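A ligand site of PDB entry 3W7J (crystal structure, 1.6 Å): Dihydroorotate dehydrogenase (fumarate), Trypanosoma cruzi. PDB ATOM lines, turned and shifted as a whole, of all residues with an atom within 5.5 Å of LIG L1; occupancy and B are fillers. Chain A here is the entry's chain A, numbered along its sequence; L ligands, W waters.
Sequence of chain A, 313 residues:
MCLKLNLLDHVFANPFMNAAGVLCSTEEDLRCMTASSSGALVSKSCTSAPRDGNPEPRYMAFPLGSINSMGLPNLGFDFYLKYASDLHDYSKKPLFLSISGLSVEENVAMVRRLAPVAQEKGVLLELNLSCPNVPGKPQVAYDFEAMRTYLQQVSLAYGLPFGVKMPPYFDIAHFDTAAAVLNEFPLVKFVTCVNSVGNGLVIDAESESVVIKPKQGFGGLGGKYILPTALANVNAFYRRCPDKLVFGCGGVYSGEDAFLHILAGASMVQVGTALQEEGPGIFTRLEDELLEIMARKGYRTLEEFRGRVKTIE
OG1 of Thr 273 lies within hydrogen-bond range of OG of Ser 66, 2.7 Å away. The side-chain hydroxyl of Ser 45 sits at hydrogen-bond distance from the side-chain hydroxyl of Ser 98 (2.6 Å). O of Cys 249 is in hydrogen-bond range of N of Val 194 (2.8 Å). The side-chain amide nitrogen of Asn 195 sits at hydrogen-bond distance from the side-chain amide oxygen of Asn 128, at 3.2 Å. The side-chain hydroxyl (OG) of Ser 196 lies within hydrogen-bond range of the side-chain amide oxygen (OD1) of Asn 195 (3.3 Å). The backbone NH of Ala 19 sits at hydrogen-bond distance from the backbone carbonyl oxygen of Val 271 (2.9 Å). The side-chain sulfur of Cys 249 is in hydrogen-bond range of the side-chain amide oxygen of Gln 270 (3.6 Å). The backbone carbonyl oxygen (O) of Gly 222 lies within hydrogen-bond range of the backbone NH (N) of Ser 66, at 2.9 Å.
An oxygen (O9) of LIG L1 lies within hydrogen-bond range of the backbone NH of Thr 273, at 2.8 Å. OG1 of Thr 273 sits at hydrogen-bond distance from O9 of LIG L1 (2.7 Å). The side-chain amino group (NZ) of Lys 44 sits at hydrogen-bond distance from an oxygen (O2) of LIG L1, 2.7 Å away. N of Gly 223 lies within hydrogen-bond range of O8 of LIG L1, at 2.7 Å. OG of Ser 45 is in hydrogen-bond range of N2 of LIG L1, at 2.7 Å. N of Ala 20 is in hydrogen-bond range of O3 of LIG L1 (3.5 Å). An oxygen (O3) of LIG L1 lies within hydrogen-bond range of the backbone carbonyl oxygen (O) of Ala 20, at 2.8 Å. The side-chain amino group (NZ) of Lys 165 lies within hydrogen-bond range of an oxygen (O3) of LIG L1 (2.9 Å). N of Gly 251 lies within hydrogen-bond range of O8 of LIG L1, at 2.9 Å. N of Gly 272 is in hydrogen-bond range of O7 of LIG L1 (2.9 Å). O of Val 194 sits at hydrogen-bond distance from O4 of LIG L1 (2.9 Å). An oxygen (O1) of LIG L1 is in hydrogen-bond range of the side-chain amide nitrogen (ND2) of Asn 195. An oxygen (O6) of LIG L1 sits at hydrogen-bond distance from the side-chain sulfur (SG) of Cys 249 (3.4 Å). NZ of Lys 44 is in salt-bridge range of O2 of LG2 L2 (3.3 Å). The side-chain amide oxygen of Asn 195 is in hydrogen-bond range of a nitrogen (N2) of LG2 L2. An oxygen (O3) of LG2 L2 is in hydrogen-bond range of the side-chain amide nitrogen (ND2) of Asn 68, at 2.9 Å. An oxygen (O4) of LG2 L2 lies within hydrogen-bond range of the side-chain amide nitrogen (ND2) of Asn 128. The backbone NH of Met 70 sits at hydrogen-bond distance from an oxygen (O1) of LG2 L2 (3.1 Å). OG of Ser 196 lies within hydrogen-bond range of O3 of LG2 L2, at 2.7 Å. N of Leu 72 is in hydrogen-bond range of O2 of LG2 L2 (2.8 Å).
Merely in contact with LIG L1: Ala 19 (3.2 Å), Gly 21 (3.3 Å), Tyr 59 (3.8 Å), Asn 68 (3.5 Å), Met 70 (3.8 Å), Asn 128 (3.7 Å), Ser 196 (3.9 Å), Gly 222 (3.6 Å), Ile 226 (3.6 Å), Gly 250 (3.4 Å) and Val 271 (3.98 Å). Of the 32 residues printed, 22 come within 4 Å of LIG L1.
A nitrogen (N1) of LIG L1 sits close to a nitrogen (N2) of LG2 L2, 3.4 Å away.
Water W1 lies within hydrogen-bond range of an oxygen (O7) of LIG L1 (2.7 Å), the backbone NH (N) of Ala 274 (2.9 Å), the backbone carbonyl oxygen (O) of Val 252 (3.0 Å) and the backbone NH (N) of Thr 273 (3.5 Å). Water W2 lies within hydrogen-bond range of the side-chain hydroxyl (OG) of Ser 98, the side-chain carboxylate (OE1) of Glu 126 and an oxygen (O1) of LIG L1.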
ATOM      1  N   ALA A  19      -7.695  -7.664  -1.542  1.00  0.00           N
ATOM      2  CA  ALA A  19      -6.384  -7.845  -2.144  1.00  0.00           C
ATOM      3  C   ALA A  19      -6.431  -8.799  -3.324  1.00  0.00           C
ATOM      4  O   ALA A  19      -7.163  -9.808  -3.266  1.00  0.00           O
ATOM      5  CB  ALA A  19      -5.373  -8.339  -1.105  1.00  0.00           C
ATOM      6  N   ALA A  20      -5.705  -8.545  -4.395  1.00  0.00           N
ATOM      7  CA  ALA A  20      -5.764  -9.444  -5.507  1.00  0.00           C
ATOM      8  C   ALA A  20      -5.489 -10.861  -5.043  1.00  0.00           C
ATOM      9  O   ALA A  20      -4.566 -11.130  -4.243  1.00  0.00           O
ATOM     10  CB  ALA A  20      -4.822  -9.010  -6.609  1.00  0.00           C
ATOM     11  N   GLY A  21      -6.249 -11.782  -5.599  1.00  0.00           N
ATOM     12  CA  GLY A  21      -6.108 -13.151  -5.251  1.00  0.00           C
ATOM     13  C   GLY A  21      -7.134 -13.664  -4.290  1.00  0.00           C
ATOM     14  O   GLY A  21      -7.390 -14.874  -4.243  1.00  0.00           O
ATOM     15  N   VAL A  22      -7.675 -12.804  -3.453  1.00  0.00           N
ATOM     16  CA  VAL A  22      -8.640 -13.231  -2.435  1.00  0.00           C
ATOM     17  C   VAL A  22     -10.022 -12.833  -2.880  1.00  0.00           C
ATOM     18  O   VAL A  22     -10.306 -11.699  -3.185  1.00  0.00           O
ATOM     19  CB  VAL A  22      -8.274 -12.624  -1.086  1.00  0.00           C
ATOM     20  CG1 VAL A  22      -9.358 -12.914  -0.073  1.00  0.00           C
ATOM     21  CG2 VAL A  22      -6.867 -13.083  -0.712  1.00  0.00           C
ATOM     22  N   LYS A  44      -8.801 -11.433  -9.741  1.00  0.00           N
ATOM     23  CA  LYS A  44      -7.657 -12.249  -9.584  1.00  0.00           C
ATOM     24  C   LYS A  44      -6.629 -12.005 -10.694  1.00  0.00           C
ATOM     25  O   LYS A  44      -6.999 -11.951 -11.868  1.00  0.00           O
ATOM     26  CB  LYS A  44      -8.093 -13.705  -9.635  1.00  0.00           C
ATOM     27  CG  LYS A  44      -6.921 -14.667  -9.737  1.00  0.00           C
ATOM     28  CD  LYS A  44      -6.034 -14.884  -8.493  1.00  0.00           C
ATOM     29  CE  LYS A  44      -4.642 -15.557  -8.773  1.00  0.00           C
ATOM     30  NZ  LYS A  44      -3.684 -15.870  -7.555  1.00  0.00           N
ATOM     31  N   SER A  45      -5.367 -11.939 -10.293  1.00  0.00           N
ATOM     32  CA  SER A  45      -4.270 -11.743 -11.287  1.00  0.00           C
ATOM     33  C   SER A  45      -4.474 -12.785 -12.366  1.00  0.00           C
ATOM     34  O   SER A  45      -4.584 -13.941 -12.066  1.00  0.00           O
ATOM     35  CB  SER A  45      -2.920 -11.821 -10.735  1.00  0.00           C
ATOM     36  OG  SER A  45      -2.771 -10.709  -9.833  1.00  0.00           O
ATOM     37  N   TYR A  59      -2.480 -23.061   0.304  1.00  0.00           N
ATOM     38  CA  TYR A  59      -2.759 -21.910   1.185  1.00  0.00           C
ATOM     39  C   TYR A  59      -3.066 -22.506   2.537  1.00  0.00           C
ATOM     40  O   TYR A  59      -3.876 -23.436   2.652  1.00  0.00           O
ATOM     41  CB  TYR A  59      -3.974 -21.154   0.665  1.00  0.00           C
ATOM     42  CG  TYR A  59      -4.499 -20.080   1.653  1.00  0.00           C
ATOM     43  CD1 TYR A  59      -3.957 -18.830   1.737  1.00  0.00           C
ATOM     44  CD2 TYR A  59      -5.474 -20.399   2.593  1.00  0.00           C
ATOM     45  CE1 TYR A  59      -4.401 -17.902   2.644  1.00  0.00           C
ATOM     46  CE2 TYR A  59      -5.911 -19.459   3.535  1.00  0.00           C
ATOM     47  CZ  TYR A  59      -5.385 -18.235   3.573  1.00  0.00           C
ATOM     48  OH  TYR A  59      -5.838 -17.255   4.456  1.00  0.00           O
ATOM     49  N   SER A  66      -0.883 -15.992   7.055  1.00  0.00           N
ATOM     50  CA  SER A  66      -1.078 -17.043   6.074  1.00  0.00           C
ATOM     51  C   SER A  66       0.247 -17.227   5.258  1.00  0.00           C
ATOM     52  O   SER A  66       1.149 -16.386   5.201  1.00  0.00           O
ATOM     53  CB  SER A  66      -2.196 -16.706   5.110  1.00  0.00           C
ATOM     54  OG  SER A  66      -1.831 -15.551   4.257  1.00  0.00           O
ATOM     55  N   ASN A  68       1.198 -18.933   1.211  1.00  0.00           N
ATOM     56  CA  ASN A  68       0.579 -19.462  -0.004  1.00  0.00           C
ATOM     57  C   ASN A  68       1.644 -19.670  -1.071  1.00  0.00           C
ATOM     58  O   ASN A  68       2.557 -18.877  -1.261  1.00  0.00           O
ATOM     59  CB  ASN A  68      -0.573 -18.609  -0.504  1.00  0.00           C
ATOM     60  CG  ASN A  68      -0.132 -17.485  -1.380  1.00  0.00           C
ATOM     61  OD1 ASN A  68       0.107 -17.701  -2.587  1.00  0.00           O
ATOM     62  ND2 ASN A  68       0.024 -16.305  -0.815  1.00  0.00           N
ATOM     63  N   MET A  70       0.029 -20.359  -4.378  1.00  0.00           N
ATOM     64  CA  MET A  70      -1.067 -20.688  -5.264  1.00  0.00           C
ATOM     65  C   MET A  70      -0.656 -21.091  -6.670  1.00  0.00           C
ATOM     66  O   MET A  70      -1.247 -22.021  -7.285  1.00  0.00           O
ATOM     67  CB  MET A  70      -2.051 -19.591  -5.333  1.00  0.00           C
ATOM     68  CG  MET A  70      -2.676 -19.073  -4.082  1.00  0.00           C
ATOM     69  SD  MET A  70      -3.458 -20.304  -3.052  1.00  0.00           S
ATOM     70  CE  MET A  70      -4.911 -20.592  -3.966  1.00  0.00           C
ATOM     71  N   LEU A  72      -0.717 -18.925  -9.300  1.00  0.00           N
ATOM     72  CA  LEU A  72      -1.496 -18.188 -10.225  1.00  0.00           C
ATOM     73  C   LEU A  72      -2.625 -18.969 -10.876  1.00  0.00           C
ATOM     74  O   LEU A  72      -2.870 -18.823 -12.111  1.00  0.00           O
ATOM     75  CB  LEU A  72      -0.581 -17.508 -11.257  1.00  0.00           C
ATOM     76  CG  LEU A  72      -1.022 -16.224 -11.982  1.00  0.00           C
ATOM     77  CD1 LEU A  72      -1.646 -15.178 -11.096  1.00  0.00           C
ATOM     78  CD2 LEU A  72       0.261 -15.666 -12.625  1.00  0.00           C
ATOM     79  N   SER A  98      -6.509  -7.080 -12.259  1.00  0.00           N
ATOM     80  CA  SER A  98      -5.071  -7.345 -12.057  1.00  0.00           C
ATOM     81  C   SER A  98      -4.575  -8.258 -13.103  1.00  0.00           C
ATOM     82  O   SER A  98      -5.228  -9.235 -13.434  1.00  0.00           O
ATOM     83  CB  SER A  98      -4.830  -7.975 -10.663  1.00  0.00           C
ATOM     84  OG  SER A  98      -3.462  -8.354 -10.530  1.00  0.00           O
ATOM     85  N   GLU A 126      -4.308  -2.982 -12.551  1.00  0.00           N
ATOM     86  CA  GLU A 126      -3.252  -3.208 -11.549  1.00  0.00           C
ATOM     87  C   GLU A 126      -2.321  -4.241 -12.174  1.00  0.00           C
ATOM     88  O   GLU A 126      -2.643  -5.430 -12.378  1.00  0.00           O
ATOM     89  CB  GLU A 126      -3.798  -3.599 -10.172  1.00  0.00           C
ATOM     90  CG  GLU A 126      -2.646  -3.735  -9.111  1.00  0.00           C
ATOM     91  CD  GLU A 126      -3.187  -4.034  -7.709  1.00  0.00           C
ATOM     92  OE1 GLU A 126      -3.415  -5.249  -7.454  1.00  0.00           O
ATOM     93  OE2 GLU A 126      -3.491  -3.177  -6.792  1.00  0.00           O
ATOM     94  N   ASN A 128       0.725  -6.653 -11.850  1.00  0.00           N
ATOM     95  CA  ASN A 128       1.510  -7.291 -10.780  1.00  0.00           C
ATOM     96  C   ASN A 128       2.920  -7.499 -11.172  1.00  0.00           C
ATOM     97  O   ASN A 128       3.216  -8.238 -12.071  1.00  0.00           O
ATOM     98  CB  ASN A 128       0.915  -8.662 -10.417  1.00  0.00           C
ATOM     99  CG  ASN A 128       1.644  -9.305  -9.236  1.00  0.00           C
ATOM    100  OD1 ASN A 128       2.296  -8.698  -8.413  1.00  0.00           O
ATOM    101  ND2 ASN A 128       1.532 -10.596  -9.204  1.00  0.00           N
ATOM    102  N   LYS A 165       1.430  -3.404  -8.614  1.00  0.00           N
ATOM    103  CA  LYS A 165       1.502  -4.114  -7.325  1.00  0.00           C
ATOM    104  C   LYS A 165       2.948  -4.521  -7.053  1.00  0.00           C
ATOM    105  O   LYS A 165       3.605  -5.212  -7.877  1.00  0.00           O
ATOM    106  CB  LYS A 165       0.643  -5.384  -7.428  1.00  0.00           C
ATOM    107  CG  LYS A 165       0.616  -6.247  -6.149  1.00  0.00           C
ATOM    108  CD  LYS A 165      -0.214  -5.675  -5.019  1.00  0.00           C
ATOM    109  CE  LYS A 165      -0.562  -6.622  -3.896  1.00  0.00           C
ATOM    110  NZ  LYS A 165      -1.466  -7.674  -4.269  1.00  0.00           N
ATOM    111  N   VAL A 194       1.818  -3.830  -0.033  1.00  0.00           N
ATOM    112  CA  VAL A 194       2.754  -4.771  -0.634  1.00  0.00           C
ATOM    113  C   VAL A 194       2.041  -6.029  -1.009  1.00  0.00           C
ATOM    114  O   VAL A 194       0.968  -6.427  -0.421  1.00  0.00           O
ATOM    115  CB  VAL A 194       3.957  -5.117   0.306  1.00  0.00           C
ATOM    116  CG1 VAL A 194       4.746  -3.816   0.503  1.00  0.00           C
ATOM    117  CG2 VAL A 194       3.457  -5.625   1.632  1.00  0.00           C
ATOM    118  N   ASN A 195       2.640  -6.726  -1.962  1.00  0.00           N
ATOM    119  CA  ASN A 195       2.405  -8.194  -2.151  1.00  0.00           C
ATOM    120  C   ASN A 195       2.926  -9.024  -0.919  1.00  0.00           C
ATOM    121  O   ASN A 195       3.567  -8.445   0.006  1.00  0.00           O
ATOM    122  CB  ASN A 195       3.030  -8.660  -3.470  1.00  0.00           C
ATOM    123  CG  ASN A 195       2.211  -9.755  -4.139  1.00  0.00           C
ATOM    124  OD1 ASN A 195       1.941 -10.796  -3.499  1.00  0.00           O
ATOM    125  ND2 ASN A 195       1.874  -9.585  -5.420  1.00  0.00           N
ATOM    126  N   SER A 196       2.775 -10.319  -0.961  1.00  0.00           N
ATOM    127  CA  SER A 196       3.236 -11.127   0.145  1.00  0.00           C
ATOM    128  C   SER A 196       4.751 -11.051   0.390  1.00  0.00           C
ATOM    129  O   SER A 196       5.472 -10.802  -0.446  1.00  0.00           O
ATOM    130  CB  SER A 196       2.732 -12.590  -0.045  1.00  0.00           C
ATOM    131  OG  SER A 196       3.055 -13.031  -1.269  1.00  0.00           O
ATOM    132  N   LEU A 221       4.069 -14.850   2.514  1.00  0.00           N
ATOM    133  CA  LEU A 221       3.458 -14.615   3.810  1.00  0.00           C
ATOM    134  C   LEU A 221       2.559 -13.420   3.780  1.00  0.00           C
ATOM    135  O   LEU A 221       2.928 -12.373   3.199  1.00  0.00           O
ATOM    136  CB  LEU A 221       4.543 -14.353   4.885  1.00  0.00           C
ATOM    137  CG  LEU A 221       5.593 -15.454   5.128  1.00  0.00           C
ATOM    138  CD1 LEU A 221       6.681 -14.958   6.042  1.00  0.00           C
ATOM    139  CD2 LEU A 221       4.959 -16.689   5.645  1.00  0.00           C
ATOM    140  N   GLY A 222       1.428 -13.545   4.430  1.00  0.00           N
ATOM    141  CA  GLY A 222       0.527 -12.418   4.623  1.00  0.00           C
ATOM    142  C   GLY A 222       0.018 -12.363   6.033  1.00  0.00           C
ATOM    143  O   GLY A 222       0.296 -13.300   6.812  1.00  0.00           O
ATOM    144  N   GLY A 223      -0.677 -11.321   6.369  1.00  0.00           N
ATOM    145  CA  GLY A 223      -1.330 -11.185   7.608  1.00  0.00           C
ATOM    146  C   GLY A 223      -0.518 -10.464   8.722  1.00  0.00           C
ATOM    147  O   GLY A 223       0.260  -9.575   8.372  1.00  0.00           O
ATOM    148  N   ILE A 226       3.203  -9.350   8.634  1.00  0.00           N
ATOM    149  CA  ILE A 226       3.747  -8.436   7.629  1.00  0.00           C
ATOM    150  C   ILE A 226       3.314  -6.990   7.766  1.00  0.00           C
ATOM    151  O   ILE A 226       3.772  -6.144   7.019  1.00  0.00           O
ATOM    152  CB  ILE A 226       3.517  -8.941   6.217  1.00  0.00           C
ATOM    153  CG1 ILE A 226       2.131  -8.614   5.701  1.00  0.00           C
ATOM    154  CG2 ILE A 226       3.927 -10.399   6.097  1.00  0.00           C
ATOM    155  CD1 ILE A 226       2.045  -8.691   4.195  1.00  0.00           C
ATOM    156  N   CYS A 249      -1.515  -2.484   1.375  1.00  0.00           N
ATOM    157  CA  CYS A 249      -1.962  -3.873   1.488  1.00  0.00           C
ATOM    158  C   CYS A 249      -0.974  -4.577   2.397  1.00  0.00           C
ATOM    159  O   CYS A 249       0.247  -4.426   2.253  1.00  0.00           O
ATOM    160  CB  CYS A 249      -1.969  -4.495   0.133  1.00  0.00           C
ATOM    161  SG  CYS A 249      -2.639  -6.181   0.101  1.00  0.00           S
ATOM    162  N   GLY A 250      -1.456  -5.278   3.420  1.00  0.00           N
ATOM    163  CA  GLY A 250      -0.628  -6.138   4.281  1.00  0.00           C
ATOM    164  C   GLY A 250      -1.020  -5.959   5.723  1.00  0.00           C
ATOM    165  O   GLY A 250      -0.917  -4.878   6.276  1.00  0.00           O
ATOM    166  N   GLY A 251      -1.513  -7.042   6.311  1.00  0.00           N
ATOM    167  CA  GLY A 251      -1.710  -7.073   7.715  1.00  0.00           C
ATOM    168  C   GLY A 251      -2.903  -6.347   8.187  1.00  0.00           C
ATOM    169  O   GLY A 251      -2.962  -6.090   9.410  1.00  0.00           O
ATOM    170  N   VAL A 252      -3.879  -6.030   7.352  1.00  0.00           N
ATOM    171  CA  VAL A 252      -5.093  -5.352   7.849  1.00  0.00           C
ATOM    172  C   VAL A 252      -6.083  -6.330   8.386  1.00  0.00           C
ATOM    173  O   VAL A 252      -6.633  -7.097   7.576  1.00  0.00           O
ATOM    174  CB  VAL A 252      -5.721  -4.480   6.709  1.00  0.00           C
ATOM    175  CG1 VAL A 252      -7.007  -3.809   7.183  1.00  0.00           C
ATOM    176  CG2 VAL A 252      -4.723  -3.393   6.281  1.00  0.00           C
ATOM    177  N   GLN A 270      -6.229  -2.402   1.010  1.00  0.00           N
ATOM    178  CA  GLN A 270      -6.629  -3.752   0.508  1.00  0.00           C
ATOM    179  C   GLN A 270      -6.520  -4.759   1.673  1.00  0.00           C
ATOM    180  O   GLN A 270      -5.664  -4.620   2.530  1.00  0.00           O
ATOM    181  CB  GLN A 270      -5.730  -4.191  -0.653  1.00  0.00           C
ATOM    182  CG  GLN A 270      -5.640  -3.157  -1.725  1.00  0.00           C
ATOM    183  CD  GLN A 270      -4.918  -3.648  -2.928  1.00  0.00           C
ATOM    184  OE1 GLN A 270      -4.133  -4.600  -2.824  1.00  0.00           O
ATOM    185  NE2 GLN A 270      -5.179  -3.024  -4.090  1.00  0.00           N
ATOM    186  N   VAL A 271      -7.323  -5.834   1.619  1.00  0.00           N
ATOM    187  CA  VAL A 271      -7.482  -6.787   2.662  1.00  0.00           C
ATOM    188  C   VAL A 271      -7.360  -8.154   2.014  1.00  0.00           C
ATOM    189  O   VAL A 271      -8.204  -8.513   1.215  1.00  0.00           O
ATOM    190  CB  VAL A 271      -8.817  -6.626   3.425  1.00  0.00           C
ATOM    191  CG1 VAL A 271      -8.760  -7.508   4.638  1.00  0.00           C
ATOM    192  CG2 VAL A 271      -9.045  -5.167   3.778  1.00  0.00           C
ATOM    193  N   GLY A 272      -6.349  -8.912   2.415  1.00  0.00           N
ATOM    194  CA  GLY A 272      -6.068 -10.241   1.843  1.00  0.00           C
ATOM    195  C   GLY A 272      -6.426 -11.310   2.893  1.00  0.00           C
ATOM    196  O   GLY A 272      -7.558 -11.751   2.972  1.00  0.00           O
ATOM    197  N   THR A 273      -5.418 -11.785   3.629  1.00  0.00           N
ATOM    198  CA  THR A 273      -5.568 -12.830   4.620  1.00  0.00           C
ATOM    199  C   THR A 273      -6.817 -12.676   5.468  1.00  0.00           C
ATOM    200  O   THR A 273      -7.560 -13.603   5.613  1.00  0.00           O
ATOM    201  CB  THR A 273      -4.309 -12.901   5.467  1.00  0.00           C
ATOM    202  OG1 THR A 273      -3.160 -13.234   4.643  1.00  0.00           O
ATOM    203  CG2 THR A 273      -4.427 -14.004   6.487  1.00  0.00           C
ATOM    204  N   ALA A 274      -7.020 -11.517   6.030  1.00  0.00           N
ATOM    205  CA  ALA A 274      -8.126 -11.331   6.992  1.00  0.00           C
ATOM    206  C   ALA A 274      -9.436 -11.561   6.290  1.00  0.00           C
ATOM    207  O   ALA A 274     -10.371 -12.033   6.913  1.00  0.00           O
ATOM    208  CB  ALA A 274      -8.064  -9.925   7.617  1.00  0.00           C
ATOM    209  N   GLN A 276      -9.843 -13.494   3.502  1.00  0.00           N
ATOM    210  CA  GLN A 276      -9.855 -14.920   3.311  1.00  0.00           C
ATOM    211  C   GLN A 276     -10.377 -15.675   4.514  1.00  0.00           C
ATOM    212  O   GLN A 276     -11.202 -16.580   4.384  1.00  0.00           O
ATOM    213  CB  GLN A 276      -8.529 -15.431   2.851  1.00  0.00           C
ATOM    214  CG  GLN A 276      -8.468 -16.909   2.552  1.00  0.00           C
ATOM    215  CD  GLN A 276      -9.381 -17.358   1.464  1.00  0.00           C
ATOM    216  OE1 GLN A 276      -9.971 -18.500   1.521  1.00  0.00           O
ATOM    217  NE2 GLN A 276      -9.412 -16.618   0.454  1.00  0.00           N
HETATM  218  N1  LIG L   1      -1.304 -10.766  -5.074  1.00  0.00           N
HETATM  219  C1  LIG L   1      -1.438 -10.424  -6.346  1.00  0.00           C
HETATM  220  O1  LIG L   1      -1.132  -9.293  -6.725  1.00  0.00           O
HETATM  221  N2  LIG L   1      -2.029 -11.230  -7.238  1.00  0.00           N
HETATM  222  C2  LIG L   1      -2.534 -12.438  -6.885  1.00  0.00           C
HETATM  223  O2  LIG L   1      -3.102 -13.217  -7.739  1.00  0.00           O
HETATM  224  C3  LIG L   1      -2.387 -12.851  -5.550  1.00  0.00           C
HETATM  225  N3  LIG L   1      -2.920 -14.020  -5.132  1.00  0.00           N
HETATM  226  C4  LIG L   1      -2.973 -14.265  -3.772  1.00  0.00           C
HETATM  227  C5  LIG L   1      -3.623 -15.415  -3.316  1.00  0.00           C
HETATM  228  C6  LIG L   1      -3.764 -15.723  -2.003  1.00  0.00           C
HETATM  229  C7  LIG L   1      -4.421 -16.966  -1.493  1.00  0.00           C
HETATM  230  C8  LIG L   1      -3.127 -14.819  -1.038  1.00  0.00           C
HETATM  231  C9  LIG L   1      -3.211 -15.062   0.403  1.00  0.00           C
HETATM  232  C10 LIG L   1      -2.462 -13.718  -1.478  1.00  0.00           C
HETATM  233  C11 LIG L   1      -2.364 -13.363  -2.817  1.00  0.00           C
HETATM  234  N4  LIG L   1      -1.737 -12.190  -3.301  1.00  0.00           N
HETATM  235  C12 LIG L   1      -1.803 -11.899  -4.620  1.00  0.00           C
HETATM  236  C13 LIG L   1      -1.182 -11.249  -2.371  1.00  0.00           C
HETATM  237  C14 LIG L   1      -2.250 -10.388  -1.700  1.00  0.00           C
HETATM  238  O3  LIG L   1      -2.857  -9.615  -2.710  1.00  0.00           O
HETATM  239  C15 LIG L   1      -1.635  -9.526  -0.642  1.00  0.00           C
HETATM  240  O4  LIG L   1      -0.682  -8.657  -1.340  1.00  0.00           O
HETATM  241  C16 LIG L   1      -0.899 -10.289   0.466  1.00  0.00           C
HETATM  242  O5  LIG L   1      -1.691 -11.405   0.849  1.00  0.00           O
HETATM  243  C17 LIG L   1      -0.717  -9.357   1.728  1.00  0.00           C
HETATM  244  O6  LIG L   1      -1.933  -8.807   2.210  1.00  0.00           O
HETATM  245  P1  LIG L   1      -2.537  -9.475   3.574  1.00  0.00           P
HETATM  246  O7  LIG L   1      -3.832  -8.702   3.771  1.00  0.00           O
HETATM  247  O8  LIG L   1      -1.506  -9.362   4.652  1.00  0.00           O
HETATM  248  O9  LIG L   1      -2.733 -10.988   3.263  1.00  0.00           O
HETATM  249  O1  LG2 L   2       0.868 -17.806  -5.902  1.00  0.00           O
HETATM  250  C1  LG2 L   2       0.205 -16.897  -6.389  1.00  0.00           C
HETATM  251  O2  LG2 L   2      -0.652 -17.046  -7.288  1.00  0.00           O
HETATM  252  C2  LG2 L   2       0.509 -15.537  -5.873  1.00  0.00           C
HETATM  253  N1  LG2 L   2       0.528 -15.449  -4.475  1.00  0.00           N
HETATM  254  C3  LG2 L   2       0.822 -14.254  -3.844  1.00  0.00           C
HETATM  255  O3  LG2 L   2       0.951 -14.184  -2.608  1.00  0.00           O
HETATM  256  N2  LG2 L   2       1.069 -13.206  -4.621  1.00  0.00           N
HETATM  257  C4  LG2 L   2       0.996 -13.198  -6.045  1.00  0.00           C
HETATM  258  O4  LG2 L   2       1.265 -12.173  -6.662  1.00  0.00           O
HETATM  259  C5  LG2 L   2       0.691 -14.419  -6.651  1.00  0.00           C
HETATM  260  C6  LG2 L   2       0.716 -14.447  -8.092  1.00  0.00           C
HETATM  261  C7  LG2 L   2       2.198 -14.446  -8.803  1.00  0.00           C
HETATM  262  C8  LG2 L   2       2.768 -15.788  -8.896  1.00  0.00           C
HETATM  263  C9  LG2 L   2       2.853 -16.531 -10.094  1.00  0.00           C
HETATM  264  C10 LG2 L   2       3.424 -17.854  -9.970  1.00  0.00           C
HETATM  265  C11 LG2 L   2       3.420 -18.726 -11.017  1.00  0.00           C
HETATM  266  C12 LG2 L   2       3.987 -19.997 -10.846  1.00  0.00           C
HETATM  267  C13 LG2 L   2       4.479 -20.479  -9.620  1.00  0.00           C
HETATM  268  C14 LG2 L   2       5.076 -21.794  -9.472  1.00  0.00           C
HETATM  269  O5  LG2 L   2       5.343 -22.363 -10.572  1.00  0.00           O
HETATM  270  O6  LG2 L   2       5.216 -22.399  -8.342  1.00  0.00           O
HETATM  271  C15 LG2 L   2       4.426 -19.678  -8.581  1.00  0.00           C
HETATM  272  C16 LG2 L   2       3.840 -18.394  -8.753  1.00  0.00           C
HETATM  273  C17 LG2 L   2       3.872 -17.653  -7.670  1.00  0.00           C
HETATM  274  C18 LG2 L   2       3.285 -16.380  -7.751  1.00  0.00           C
HETATM  275  O   HOH W   1      -5.252  -9.221   5.976  1.00  0.00           O
HETATM  276  O   HOH W   2      -2.123  -7.337  -8.579  1.00  0.00           O
HETATM  277  O   HOH W   3      -4.048  -6.137   4.314  1.00  0.00           O
HETATM  278  O   HOH W   4       0.037 -13.221   1.009  1.00  0.00           O
